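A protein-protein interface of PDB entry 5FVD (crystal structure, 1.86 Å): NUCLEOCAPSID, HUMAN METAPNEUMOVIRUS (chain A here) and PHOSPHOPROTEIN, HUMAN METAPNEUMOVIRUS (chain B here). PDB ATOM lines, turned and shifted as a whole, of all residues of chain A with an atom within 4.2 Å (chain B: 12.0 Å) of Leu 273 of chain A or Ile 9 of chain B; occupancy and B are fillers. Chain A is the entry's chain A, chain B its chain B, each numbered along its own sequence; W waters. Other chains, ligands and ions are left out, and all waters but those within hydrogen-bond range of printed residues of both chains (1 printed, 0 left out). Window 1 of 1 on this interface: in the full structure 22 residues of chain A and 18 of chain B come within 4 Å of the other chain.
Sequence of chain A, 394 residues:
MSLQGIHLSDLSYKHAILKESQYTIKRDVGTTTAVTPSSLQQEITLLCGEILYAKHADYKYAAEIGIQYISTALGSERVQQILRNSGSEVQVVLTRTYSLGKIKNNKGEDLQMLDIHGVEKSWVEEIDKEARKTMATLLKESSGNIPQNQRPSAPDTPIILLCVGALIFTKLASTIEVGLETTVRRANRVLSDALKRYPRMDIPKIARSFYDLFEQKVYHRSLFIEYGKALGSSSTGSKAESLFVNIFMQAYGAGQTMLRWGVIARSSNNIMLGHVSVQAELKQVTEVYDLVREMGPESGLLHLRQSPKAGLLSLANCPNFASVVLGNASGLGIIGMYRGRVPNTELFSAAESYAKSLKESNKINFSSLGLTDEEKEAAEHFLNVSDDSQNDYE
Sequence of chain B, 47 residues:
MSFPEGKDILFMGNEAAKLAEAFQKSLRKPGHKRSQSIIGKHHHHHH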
ATOM      1  N   GLY A 262       4.945  16.315   4.998  1.00  0.00           N
ATOM      2  CA  GLY A 262       4.841  16.832   3.645  1.00  0.00           C
ATOM      3  C   GLY A 262       6.145  16.679   2.875  1.00  0.00           C
ATOM      4  O   GLY A 262       6.155  16.230   1.722  1.00  0.00           O
ATOM      5  N   ALA A 265       6.666  13.124   2.015  1.00  0.00           N
ATOM      6  CA  ALA A 265       5.882  12.718   0.841  1.00  0.00           C
ATOM      7  C   ALA A 265       6.637  13.004  -0.466  1.00  0.00           C
ATOM      8  O   ALA A 265       6.585  12.214  -1.412  1.00  0.00           O
ATOM      9  CB  ALA A 265       4.545  13.411   0.841  1.00  0.00           C
ATOM     10  N   ARG A 266       7.346  14.129  -0.511  1.00  0.00           N
ATOM     11  CA  ARG A 266       8.160  14.470  -1.676  1.00  0.00           C
ATOM     12  C   ARG A 266       9.414  13.591  -1.757  1.00  0.00           C
ATOM     13  O   ARG A 266       9.799  13.151  -2.847  1.00  0.00           O
ATOM     14  CB  ARG A 266       8.545  15.956  -1.642  1.00  0.00           C
ATOM     15  CG  ARG A 266       9.491  16.392  -2.758  1.00  0.00           C
ATOM     16  CD  ARG A 266       8.903  16.087  -4.129  1.00  0.00           C
ATOM     17  NE  ARG A 266       9.740  16.595  -5.209  1.00  0.00           N
ATOM     18  CZ  ARG A 266      10.828  15.973  -5.650  1.00  0.00           C
ATOM     19  NH1 ARG A 266      11.214  14.825  -5.097  1.00  0.00           N
ATOM     20  NH2 ARG A 266      11.536  16.499  -6.641  1.00  0.00           N
ATOM     21  N   ASN A 270       6.019  10.612  -3.939  1.00  0.00           N
ATOM     22  CA  ASN A 270       4.633  10.228  -4.097  1.00  0.00           C
ATOM     23  C   ASN A 270       4.026  10.983  -5.268  1.00  0.00           C
ATOM     24  O   ASN A 270       3.890  12.204  -5.215  1.00  0.00           O
ATOM     25  CB  ASN A 270       3.833  10.503  -2.822  1.00  0.00           C
ATOM     26  CG  ASN A 270       2.512   9.762  -2.814  1.00  0.00           C
ATOM     27  OD1 ASN A 270       1.696   9.925  -3.718  1.00  0.00           O
ATOM     28  ND2 ASN A 270       2.320   8.898  -1.827  1.00  0.00           N
ATOM     29  N   ILE A 271       3.647  10.258  -6.321  1.00  0.00           N
ATOM     30  CA  ILE A 271       3.218  10.912  -7.547  1.00  0.00           C
ATOM     31  C   ILE A 271       1.878  11.623  -7.384  1.00  0.00           C
ATOM     32  O   ILE A 271       1.507  12.453  -8.219  1.00  0.00           O
ATOM     33  CB  ILE A 271       3.156   9.931  -8.710  1.00  0.00           C
ATOM     34  CG1 ILE A 271       2.135   8.830  -8.436  1.00  0.00           C
ATOM     35  CG2 ILE A 271       4.546   9.348  -8.956  1.00  0.00           C
ATOM     36  CD1 ILE A 271       1.910   7.939  -9.645  1.00  0.00           C
ATOM     37  N   MET A 272       1.151  11.324  -6.315  1.00  0.00           N
ATOM     38  CA  MET A 272      -0.114  12.031  -6.100  1.00  0.00           C
ATOM     39  C   MET A 272       0.139  13.500  -5.725  1.00  0.00           C
ATOM     40  O   MET A 272      -0.784  14.325  -5.725  1.00  0.00           O
ATOM     41  CB  MET A 272      -0.962  11.338  -5.026  1.00  0.00           C
ATOM     42  CG  MET A 272      -1.421   9.934  -5.414  1.00  0.00           C
ATOM     43  SD  MET A 272      -2.093   9.784  -7.105  1.00  0.00           S
ATOM     44  CE  MET A 272      -3.598  10.756  -6.973  1.00  0.00           C
ATOM     45  N   LEU A 273       1.389  13.836  -5.416  1.00  0.00           N
ATOM     46  CA  LEU A 273       1.760  15.232  -5.217  1.00  0.00           C
ATOM     47  C   LEU A 273       1.660  16.008  -6.539  1.00  0.00           C
ATOM     48  O   LEU A 273       1.787  17.235  -6.564  1.00  0.00           O
ATOM     49  CB  LEU A 273       3.170  15.340  -4.634  1.00  0.00           C
ATOM     50  CG  LEU A 273       3.316  14.966  -3.151  1.00  0.00           C
ATOM     51  CD1 LEU A 273       4.799  14.921  -2.769  1.00  0.00           C
ATOM     52  CD2 LEU A 273       2.575  15.964  -2.267  1.00  0.00           C
ATOM     53  N   GLY A 274       1.434  15.294  -7.639  1.00  0.00           N
ATOM     54  CA  GLY A 274       1.228  15.940  -8.928  1.00  0.00           C
ATOM     55  C   GLY A 274      -0.221  16.051  -9.402  1.00  0.00           C
ATOM     56  O   GLY A 274      -0.490  16.575 -10.497  1.00  0.00           O
ATOM     57  N   HIS A 275      -1.161  15.570  -8.592  1.00  0.00           N
ATOM     58  CA  HIS A 275      -2.583  15.636  -8.955  1.00  0.00           C
ATOM     59  C   HIS A 275      -3.018  17.096  -9.168  1.00  0.00           C
ATOM     60  O   HIS A 275      -2.574  17.985  -8.445  1.00  0.00           O
ATOM     61  CB  HIS A 275      -3.442  14.964  -7.872  1.00  0.00           C
ATOM     62  CG  HIS A 275      -4.869  14.746  -8.281  1.00  0.00           C
ATOM     63  ND1 HIS A 275      -5.849  15.695  -8.101  1.00  0.00           N
ATOM     64  CD2 HIS A 275      -5.473  13.689  -8.871  1.00  0.00           C
ATOM     65  CE1 HIS A 275      -6.999  15.232  -8.560  1.00  0.00           C
ATOM     66  NE2 HIS A 275      -6.797  14.019  -9.041  1.00  0.00           N
ATOM     67  N   VAL A 278      -4.071  19.160  -6.273  1.00  0.00           N
ATOM     68  CA  VAL A 278      -2.968  19.470  -5.379  1.00  0.00           C
ATOM     69  C   VAL A 278      -2.121  20.596  -5.974  1.00  0.00           C
ATOM     70  O   VAL A 278      -1.772  21.539  -5.268  1.00  0.00           O
ATOM     71  CB  VAL A 278      -2.124  18.226  -5.090  1.00  0.00           C
ATOM     72  CG1 VAL A 278      -0.854  18.605  -4.333  1.00  0.00           C
ATOM     73  CG2 VAL A 278      -2.953  17.206  -4.305  1.00  0.00           C
ATOM     74  N   TYR A 289       4.896  26.679   3.856  1.00  0.00           N
ATOM     75  CA  TYR A 289       6.318  26.407   4.014  1.00  0.00           C
ATOM     76  C   TYR A 289       7.132  27.688   4.127  1.00  0.00           C
ATOM     77  O   TYR A 289       8.207  27.672   4.715  1.00  0.00           O
ATOM     78  CB  TYR A 289       6.823  25.511   2.873  1.00  0.00           C
ATOM     79  CG  TYR A 289       6.377  24.092   3.114  1.00  0.00           C
ATOM     80  CD1 TYR A 289       7.106  23.245   3.949  1.00  0.00           C
ATOM     81  CD2 TYR A 289       5.183  23.619   2.584  1.00  0.00           C
ATOM     82  CE1 TYR A 289       6.680  21.956   4.210  1.00  0.00           C
ATOM     83  CE2 TYR A 289       4.749  22.321   2.845  1.00  0.00           C
ATOM     84  CZ  TYR A 289       5.503  21.496   3.654  1.00  0.00           C
ATOM     85  OH  TYR A 289       5.067  20.207   3.926  1.00  0.00           O
ATOM     86  N   PHE A 321      -3.571  18.714  -0.660  1.00  0.00           N
ATOM     87  CA  PHE A 321      -2.189  18.440  -0.282  1.00  0.00           C
ATOM     88  C   PHE A 321      -2.149  17.643   1.014  1.00  0.00           C
ATOM     89  O   PHE A 321      -1.455  16.627   1.113  1.00  0.00           O
ATOM     90  CB  PHE A 321      -1.401  19.754  -0.135  1.00  0.00           C
ATOM     91  CG  PHE A 321      -0.008  19.573   0.403  1.00  0.00           C
ATOM     92  CD1 PHE A 321       0.951  18.891  -0.338  1.00  0.00           C
ATOM     93  CD2 PHE A 321       0.350  20.115   1.628  1.00  0.00           C
ATOM     94  CE1 PHE A 321       2.245  18.726   0.152  1.00  0.00           C
ATOM     95  CE2 PHE A 321       1.631  19.968   2.116  1.00  0.00           C
ATOM     96  CZ  PHE A 321       2.583  19.272   1.381  1.00  0.00           C
ATOM     97  N   VAL A 324      -2.902  13.942   0.543  1.00  0.00           N
ATOM     98  CA  VAL A 324      -1.787  13.200  -0.051  1.00  0.00           C
ATOM     99  C   VAL A 324      -0.681  13.011   0.989  1.00  0.00           C
ATOM    100  O   VAL A 324      -0.097  11.927   1.098  1.00  0.00           O
ATOM    101  CB  VAL A 324      -1.266  13.903  -1.321  1.00  0.00           C
ATOM    102  CG1 VAL A 324       0.058  13.276  -1.779  1.00  0.00           C
ATOM    103  CG2 VAL A 324      -2.322  13.808  -2.417  1.00  0.00           C
ATOM    104  N   MET B   1      16.229  19.891  10.555  1.00  0.00           N
ATOM    105  CA  MET B   1      15.179  19.754   9.546  1.00  0.00           C
ATOM    106  C   MET B   1      15.114  20.984   8.630  1.00  0.00           C
ATOM    107  O   MET B   1      14.793  22.087   9.074  1.00  0.00           O
ATOM    108  CB  MET B   1      13.818  19.520  10.216  1.00  0.00           C
ATOM    109  CG  MET B   1      12.671  19.306   9.234  1.00  0.00           C
ATOM    110  SD  MET B   1      12.874  17.825   8.218  1.00  0.00           S
ATOM    111  CE  MET B   1      11.709  18.151   6.896  1.00  0.00           C
ATOM    112  N   SER B   2      15.416  20.777   7.351  1.00  0.00           N
ATOM    113  CA  SER B   2      15.444  21.857   6.366  1.00  0.00           C
ATOM    114  C   SER B   2      14.240  21.805   5.426  1.00  0.00           C
ATOM    115  O   SER B   2      14.113  20.883   4.619  1.00  0.00           O
ATOM    116  CB  SER B   2      16.739  21.796   5.551  1.00  0.00           C
ATOM    117  OG  SER B   2      16.664  22.622   4.402  1.00  0.00           O
ATOM    118  N   PHE B   3      13.367  22.802   5.521  1.00  0.00           N
ATOM    119  CA  PHE B   3      12.143  22.811   4.722  1.00  0.00           C
ATOM    120  C   PHE B   3      12.360  23.482   3.362  1.00  0.00           C
ATOM    121  O   PHE B   3      12.886  24.593   3.285  1.00  0.00           O
ATOM    122  CB  PHE B   3      11.007  23.508   5.478  1.00  0.00           C
ATOM    123  CG  PHE B   3      10.525  22.757   6.700  1.00  0.00           C
ATOM    124  CD1 PHE B   3       9.643  21.695   6.573  1.00  0.00           C
ATOM    125  CD2 PHE B   3      10.954  23.121   7.973  1.00  0.00           C
ATOM    126  CE1 PHE B   3       9.196  21.002   7.695  1.00  0.00           C
ATOM    127  CE2 PHE B   3      10.506  22.438   9.095  1.00  0.00           C
ATOM    128  CZ  PHE B   3       9.632  21.386   8.960  1.00  0.00           C
ATOM    129  N   PRO B   4      11.995  22.786   2.278  1.00  0.00           N
ATOM    130  CA  PRO B   4      12.052  23.386   0.941  1.00  0.00           C
ATOM    131  C   PRO B   4      10.866  24.313   0.665  1.00  0.00           C
ATOM    132  O   PRO B   4       9.943  24.410   1.481  1.00  0.00           O
ATOM    133  CB  PRO B   4      12.039  22.168   0.013  1.00  0.00           C
ATOM    134  CG  PRO B   4      11.308  21.128   0.777  1.00  0.00           C
ATOM    135  CD  PRO B   4      11.623  21.361   2.235  1.00  0.00           C
ATOM    136  N   GLU B   5      10.899  25.011  -0.465  1.00  0.00           N
ATOM    137  CA  GLU B   5       9.759  25.829  -0.866  1.00  0.00           C
ATOM    138  C   GLU B   5       8.652  24.917  -1.359  1.00  0.00           C
ATOM    139  O   GLU B   5       8.914  23.782  -1.771  1.00  0.00           O
ATOM    140  CB  GLU B   5      10.151  26.829  -1.954  1.00  0.00           C
ATOM    141  CG  GLU B   5      11.246  27.787  -1.538  1.00  0.00           C
ATOM    142  CD  GLU B   5      11.711  28.666  -2.682  1.00  0.00           C
ATOM    143  OE1 GLU B   5      10.846  29.221  -3.395  1.00  0.00           O
ATOM    144  OE2 GLU B   5      12.944  28.798  -2.864  1.00  0.00           O
ATOM    145  N   GLY B   6       7.421  25.419  -1.321  1.00  0.00           N
ATOM    146  CA  GLY B   6       6.258  24.645  -1.730  1.00  0.00           C
ATOM    147  C   GLY B   6       6.336  24.127  -3.156  1.00  0.00           C
ATOM    148  O   GLY B   6       5.895  23.017  -3.449  1.00  0.00           O
ATOM    149  N   LYS B   7       6.920  24.927  -4.043  1.00  0.00           N
ATOM    150  CA  LYS B   7       7.055  24.539  -5.439  1.00  0.00           C
ATOM    151  C   LYS B   7       8.062  23.402  -5.616  1.00  0.00           C
ATOM    152  O   LYS B   7       8.140  22.795  -6.687  1.00  0.00           O
ATOM    153  CB  LYS B   7       7.476  25.743  -6.293  1.00  0.00           C
ATOM    154  CG  LYS B   7       8.870  26.275  -5.985  1.00  0.00           C
ATOM    155  CD  LYS B   7       9.212  27.453  -6.889  1.00  0.00           C
ATOM    156  CE  LYS B   7      10.585  28.027  -6.575  1.00  0.00           C
ATOM    157  NZ  LYS B   7      10.757  29.381  -7.180  1.00  0.00           N
ATOM    158  N   ASP B   8       8.849  23.130  -4.580  1.00  0.00           N
ATOM    159  CA  ASP B   8       9.813  22.038  -4.632  1.00  0.00           C
ATOM    160  C   ASP B   8       9.262  20.798  -3.928  1.00  0.00           C
ATOM    161  O   ASP B   8       9.870  19.724  -3.948  1.00  0.00           O
ATOM    162  CB  ASP B   8      11.146  22.476  -4.020  1.00  0.00           C
ATOM    163  CG  ASP B   8      11.863  23.510  -4.878  1.00  0.00           C
ATOM    164  OD1 ASP B   8      11.692  23.471  -6.117  1.00  0.00           O
ATOM    165  OD2 ASP B   8      12.595  24.361  -4.324  1.00  0.00           O
ATOM    166  N   ILE B   9       8.083  20.949  -3.334  1.00  0.00           N
ATOM    167  CA  ILE B   9       7.412  19.835  -2.698  1.00  0.00           C
ATOM    168  C   ILE B   9       6.375  19.248  -3.647  1.00  0.00           C
ATOM    169  O   ILE B   9       6.281  18.036  -3.788  1.00  0.00           O
ATOM    170  CB  ILE B   9       6.805  20.262  -1.358  1.00  0.00           C
ATOM    171  CG1 ILE B   9       7.947  20.568  -0.388  1.00  0.00           C
ATOM    172  CG2 ILE B   9       5.884  19.170  -0.790  1.00  0.00           C
ATOM    173  CD1 ILE B   9       7.536  21.100   0.953  1.00  0.00           C
ATOM    174  N   LEU B  10       5.589  20.099  -4.289  1.00  0.00           N
ATOM    175  CA  LEU B  10       4.591  19.607  -5.237  1.00  0.00           C
ATOM    176  C   LEU B  10       5.255  19.189  -6.548  1.00  0.00           C
ATOM    177  O   LEU B  10       6.350  19.627  -6.849  1.00  0.00           O
ATOM    178  CB  LEU B  10       3.522  20.671  -5.501  1.00  0.00           C
ATOM    179  CG  LEU B  10       2.779  21.211  -4.282  1.00  0.00           C
ATOM    180  CD1 LEU B  10       1.616  22.117  -4.687  1.00  0.00           C
ATOM    181  CD2 LEU B  10       2.293  20.055  -3.396  1.00  0.00           C
ATOM    182  N   PHE B  11       4.592  18.325  -7.313  1.00  0.00           N
ATOM    183  CA  PHE B  11       4.991  18.048  -8.692  1.00  0.00           C
ATOM    184  C   PHE B  11       4.113  18.856  -9.634  1.00  0.00           C
ATOM    185  O   PHE B  11       2.929  18.561  -9.794  1.00  0.00           O
ATOM    186  CB  PHE B  11       4.864  16.560  -9.022  1.00  0.00           C
ATOM    187  CG  PHE B  11       5.897  15.687  -8.356  1.00  0.00           C
ATOM    188  CD1 PHE B  11       7.241  15.802  -8.681  1.00  0.00           C
ATOM    189  CD2 PHE B  11       5.516  14.723  -7.436  1.00  0.00           C
ATOM    190  CE1 PHE B  11       8.183  14.988  -8.078  1.00  0.00           C
ATOM    191  CE2 PHE B  11       6.455  13.903  -6.833  1.00  0.00           C
ATOM    192  CZ  PHE B  11       7.788  14.035  -7.155  1.00  0.00           C
ATOM    193  N   MET B  12       4.689  19.866 -10.269  1.00  0.00           N
ATOM    194  CA  MET B  12       3.899  20.764 -11.095  1.00  0.00           C
ATOM    195  C   MET B  12       4.009  20.359 -12.551  1.00  0.00           C
ATOM    196  O   MET B  12       4.946  19.667 -12.940  1.00  0.00           O
ATOM    197  CB  MET B  12       4.352  22.214 -10.906  1.00  0.00           C
ATOM    198  CG  MET B  12       4.329  22.697  -9.461  1.00  0.00           C
ATOM    199  SD  MET B  12       2.687  22.714  -8.717  1.00  0.00           S
ATOM    200  CE  MET B  12       1.816  23.842  -9.796  1.00  0.00           C
ATOM    201  N   GLY B  13       3.051  20.800 -13.356  1.00  0.00           N
ATOM    202  CA  GLY B  13       3.104  20.547 -14.780  1.00  0.00           C
ATOM    203  C   GLY B  13       2.071  19.555 -15.263  1.00  0.00           C
ATOM    204  O   GLY B  13       1.529  18.742 -14.493  1.00  0.00           O
ATOM    205  N   ASN B  14       1.805  19.629 -16.559  1.00  0.00           N
ATOM    206  CA  ASN B  14       0.797  18.810 -17.201  1.00  0.00           C
ATOM    207  C   ASN B  14       1.142  17.332 -17.076  1.00  0.00           C
ATOM    208  O   ASN B  14       0.279  16.506 -16.793  1.00  0.00           O
ATOM    209  CB  ASN B  14       0.669  19.204 -18.674  1.00  0.00           C
ATOM    210  CG  ASN B  14      -0.735  19.035 -19.197  1.00  0.00           C
ATOM    211  OD1 ASN B  14      -1.506  18.232 -18.676  1.00  0.00           O
ATOM    212  ND2 ASN B  14      -1.076  19.787 -20.241  1.00  0.00           N
ATOM    213  N   GLU B  15       2.412  17.010 -17.290  1.00  0.00           N
ATOM    214  CA  GLU B  15       2.875  15.629 -17.225  1.00  0.00           C
ATOM    215  C   GLU B  15       2.648  15.031 -15.836  1.00  0.00           C
ATOM    216  O   GLU B  15       2.164  13.912 -15.710  1.00  0.00           O
ATOM    217  CB  GLU B  15       4.355  15.546 -17.601  1.00  0.00           C
ATOM    218  CG  GLU B  15       4.911  14.132 -17.620  1.00  0.00           C
ATOM    219  CD  GLU B  15       6.387  14.091 -17.979  1.00  0.00           C
ATOM    220  OE1 GLU B  15       6.756  14.623 -19.047  1.00  0.00           O
ATOM    221  OE2 GLU B  15       7.178  13.527 -17.193  1.00  0.00           O
ATOM    222  N   ALA B  16       3.001  15.783 -14.803  1.00  0.00           N
ATOM    223  CA  ALA B  16       2.789  15.337 -13.426  1.00  0.00           C
ATOM    224  C   ALA B  16       1.300  15.103 -13.140  1.00  0.00           C
ATOM    225  O   ALA B  16       0.932  14.158 -12.431  1.00  0.00           O
ATOM    226  CB  ALA B  16       3.373  16.348 -12.454  1.00  0.00           C
ATOM    227  N   ALA B  17       0.442  15.953 -13.698  1.00  0.00           N
ATOM    228  CA  ALA B  17      -0.998  15.790 -13.519  1.00  0.00           C
ATOM    229  C   ALA B  17      -1.488  14.507 -14.185  1.00  0.00           C
ATOM    230  O   ALA B  17      -2.242  13.739 -13.588  1.00  0.00           O
ATOM    231  CB  ALA B  17      -1.748  16.992 -14.071  1.00  0.00           C
ATOM    232  N   LYS B  18      -1.048  14.270 -15.416  1.00  0.00           N
ATOM    233  CA  LYS B  18      -1.465  13.078 -16.144  1.00  0.00           C
ATOM    234  C   LYS B  18      -0.975  11.803 -15.452  1.00  0.00           C
ATOM    235  O   LYS B  18      -1.688  10.805 -15.426  1.00  0.00           O
ATOM    236  CB  LYS B  18      -0.971  13.127 -17.594  1.00  0.00           C
ATOM    237  CG  LYS B  18      -1.685  14.162 -18.461  1.00  0.00           C
ATOM    238  CD  LYS B  18      -1.747  13.727 -19.924  1.00  0.00           C
ATOM    239  CE  LYS B  18      -0.357  13.507 -20.491  1.00  0.00           C
ATOM    240  NZ  LYS B  18      -0.388  12.926 -21.866  1.00  0.00           N
ATOM    241  N   LEU B  19       0.231  11.836 -14.893  1.00  0.00           N
ATOM    242  CA  LEU B  19       0.770  10.667 -14.198  1.00  0.00           C
ATOM    243  C   LEU B  19      -0.103  10.279 -12.999  1.00  0.00           C
ATOM    244  O   LEU B  19      -0.473   9.117 -12.843  1.00  0.00           O
ATOM    245  CB  LEU B  19       2.208  10.918 -13.733  1.00  0.00           C
ATOM    246  CG  LEU B  19       3.259  11.112 -14.828  1.00  0.00           C
ATOM    247  CD1 LEU B  19       4.610  11.527 -14.239  1.00  0.00           C
ATOM    248  CD2 LEU B  19       3.394   9.863 -15.705  1.00  0.00           C
ATOM    249  N   ALA B  20      -0.441  11.261 -12.165  1.00  0.00           N
ATOM    250  CA  ALA B  20      -1.270  11.017 -10.989  1.00  0.00           C
ATOM    251  C   ALA B  20      -2.670  10.545 -11.392  1.00  0.00           C
ATOM    252  O   ALA B  20      -3.229   9.636 -10.788  1.00  0.00           O
ATOM    253  CB  ALA B  20      -1.356  12.277 -10.122  1.00  0.00           C
ATOM    254  N   GLU B  21      -3.227  11.164 -12.423  1.00  0.00           N
ATOM    255  CA  GLU B  21      -4.535  10.773 -12.919  1.00  0.00           C
ATOM    256  C   GLU B  21      -4.537   9.309 -13.379  1.00  0.00           C
ATOM    257  O   GLU B  21      -5.459   8.550 -13.069  1.00  0.00           O
ATOM    258  CB  GLU B  21      -4.949  11.704 -14.057  1.00  0.00           C
ATOM    259  CG  GLU B  21      -6.356  11.530 -14.546  1.00  0.00           C
ATOM    260  CD  GLU B  21      -6.737  12.617 -15.528  1.00  0.00           C
ATOM    261  OE1 GLU B  21      -6.396  12.486 -16.725  1.00  0.00           O
ATOM    262  OE2 GLU B  21      -7.359  13.611 -15.096  1.00  0.00           O
ATOM    263  N   ALA B  22      -3.498   8.912 -14.107  1.00  0.00           N
ATOM    264  CA  ALA B  22      -3.417   7.547 -14.608  1.00  0.00           C
ATOM    265  C   ALA B  22      -3.329   6.540 -13.462  1.00  0.00           C
ATOM    266  O   ALA B  22      -4.023   5.521 -13.472  1.00  0.00           O
ATOM    267  CB  ALA B  22      -2.230   7.394 -15.546  1.00  0.00           C
ATOM    268  N   PHE B  23      -2.505   6.839 -12.455  1.00  0.00           N
ATOM    269  CA  PHE B  23      -2.367   5.931 -11.324  1.00  0.00           C
ATOM    270  C   PHE B  23      -3.685   5.761 -10.593  1.00  0.00           C
ATOM    271  O   PHE B  23      -4.066   4.652 -10.225  1.00  0.00           O
ATOM    272  CB  PHE B  23      -1.312   6.416 -10.332  1.00  0.00           C
ATOM    273  CG  PHE B  23      -1.212   5.552  -9.121  1.00  0.00           C
ATOM    274  CD1 PHE B  23      -0.599   4.310  -9.197  1.00  0.00           C
ATOM    275  CD2 PHE B  23      -1.756   5.957  -7.911  1.00  0.00           C
ATOM    276  CE1 PHE B  23      -0.517   3.493  -8.080  1.00  0.00           C
ATOM    277  CE2 PHE B  23      -1.681   5.141  -6.798  1.00  0.00           C
ATOM    278  CZ  PHE B  23      -1.047   3.908  -6.886  1.00  0.00           C
ATOM    279  N   GLN B  24      -4.360   6.878 -10.361  1.00  0.00           N
ATOM    280  CA  GLN B  24      -5.664   6.883  -9.717  1.00  0.00           C
ATOM    281  C   GLN B  24      -6.656   6.010 -10.485  1.00  0.00           C
ATOM    282  O   GLN B  24      -7.426   5.256  -9.889  1.00  0.00           O
ATOM    283  CB  GLN B  24      -6.189   8.307  -9.618  1.00  0.00           C
ATOM    284  CG  GLN B  24      -6.559   8.731  -8.236  1.00  0.00           C
ATOM    285  CD  GLN B  24      -7.265  10.061  -8.241  1.00  0.00           C
ATOM    286  OE1 GLN B  24      -6.908  10.959  -9.004  1.00  0.00           O
ATOM    287  NE2 GLN B  24      -8.274  10.200  -7.393  1.00  0.00           N
ATOM    288  N   LEU B  27      -6.372   2.210 -10.096  1.00  0.00           N
ATOM    289  CA  LEU B  27      -6.914   1.701  -8.837  1.00  0.00           C
ATOM    290  C   LEU B  27      -8.413   1.402  -8.932  1.00  0.00           C
ATOM    291  O   LEU B  27      -9.046   1.059  -7.926  1.00  0.00           O
ATOM    292  CB  LEU B  27      -6.654   2.702  -7.712  1.00  0.00           C
ATOM    293  CG  LEU B  27      -5.175   3.002  -7.428  1.00  0.00           C
ATOM    294  CD1 LEU B  27      -5.023   4.073  -6.352  1.00  0.00           C
ATOM    295  CD2 LEU B  27      -4.422   1.744  -7.037  1.00  0.00           C
HETATM  296  O   HOH W   1       2.699  13.144 -10.654  1.00  0.00           O
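O of Asp 8 of chain B is in hydrogen-bond range of NE of Arg 266 of chain A, at 3.4 Å.
The backbone carbonyl oxygen of Leu 273 of chain A lies within hydrogen-bond range of the backbone NH of Phe 11 of chain B, at 3.1 Å.
N of Ala 17 of chain B lies close to O of Gly 274 of chain A (3.4 Å).
A ring nitrogen (NE2) of His 275 of chain A sits at hydrogen-bond distance from the side-chain amide oxygen (OE1) of Gln 24 of chain B (3.1 Å).
The backbone carbonyl oxygen (O) of Gly 274 of chain A sits close to the backbone carbonyl oxygen (O) of Ala 16 of chain B.
O of Ala 265 of chain A is in hydrogen-bond range of N of Asn 270 of chain A (3.0 Å).
The side-chain amide oxygen (OD1) of Asn 270 of chain A is in hydrogen-bond range of the backbone NH (N) of Met 272 of chain A (3.0 Å).
Ile 271 of chain A touches Phe 23 of chain B.
Met 272 of chain A touches Ala 20 of chain B (SD to O, 3.9 Å).
Met 272 of chain A touches Phe 23 of chain B.
CE of Met 272 of chain A touches CG of Gln 24 of chain B (3.8 Å).
Leu 273 of chain A touches Ile 9 of chain B (CD1 to O, 3.6 Å).
Leu 10 of chain B touches Leu 273 of chain A (CA to O, 3.9 Å).
N of His 275 of chain A touches CB of Ala 20 of chain B, 3.6 Å away.
CE1 of Tyr 289 of chain A touches CD1 of Phe 3 of chain B, 3.8 Å away.
CB of Tyr 289 of chain A touches O of Pro 4 of chain B, at 3.6 Å.
Of chain B, only Ile 9, Leu 10 and Phe 11 come within 4 Å of Leu 273 of chain A.
Of chain A, only Gly 262 (3.9 Å), Arg 266 (3.3 Å), Leu 273 (3.6 Å), Tyr 289 (3.4 Å) and Phe 321 (3.8 Å) come within 4 Å of Ile 9 of chain B.
Gly 262 of chain A touches just one residue of chain B: Ile 9.
Arg 266 of chain A touches just these residues of chain B: Asp 8, Ile 9 and Phe 11.
Asn 270 of chain A touches just one residue of chain B: Phe 11 (3.5 Å).
Val 278 of chain A touches just one residue of chain B: Leu 10.
Of chain B, only Ile 9 and Leu 10 come within 4 Å of Phe 321 of chain A.
Printed residues of chain A within 4 Å of Gln 24 of chain B: Met 272 and His 275.
Of the printed residues of chain A, Ala 17 of chain B touches Gly 274 (3.2 Å).
Of the printed residues of chain A, Pro 4 of chain B touches Tyr 289 (3.6 Å).
Leu 27 of chain B touches none of the printed residues of chain A.
Gly 13 of chain B touches none of the printed residues of chain A.
The nearest residue of chain B that does not touch Leu 273 of chain A is Met 12 of chain B (5.4 Å).
Of the 25 printed residues of chain B, 11 touch a printed residue of chain A.
Hydrophobic or aromatic side chains of chain B that line the printed part of chain A: Phe 3, Ile 9, Leu 10, Phe 11, Ala 17, Ala 20 and Phe 23.
Of the 13 printed residues of chain A, 11 touch a printed residue of chain B.
Along chain A the printed residues that touch a printed residue of chain B span positions 262 to 321.
Among the printed residues, 24 pairs touch across the chains.
Among the printed residues, no Asp or Glu carboxylate lies within 4 Å of a Lys or Arg side-chain nitrogen of the other chain.
Water W1 bridges O of Ala 16 of chain B (2.7 Å) and O of Ile 271 of chain A (2.8 Å).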
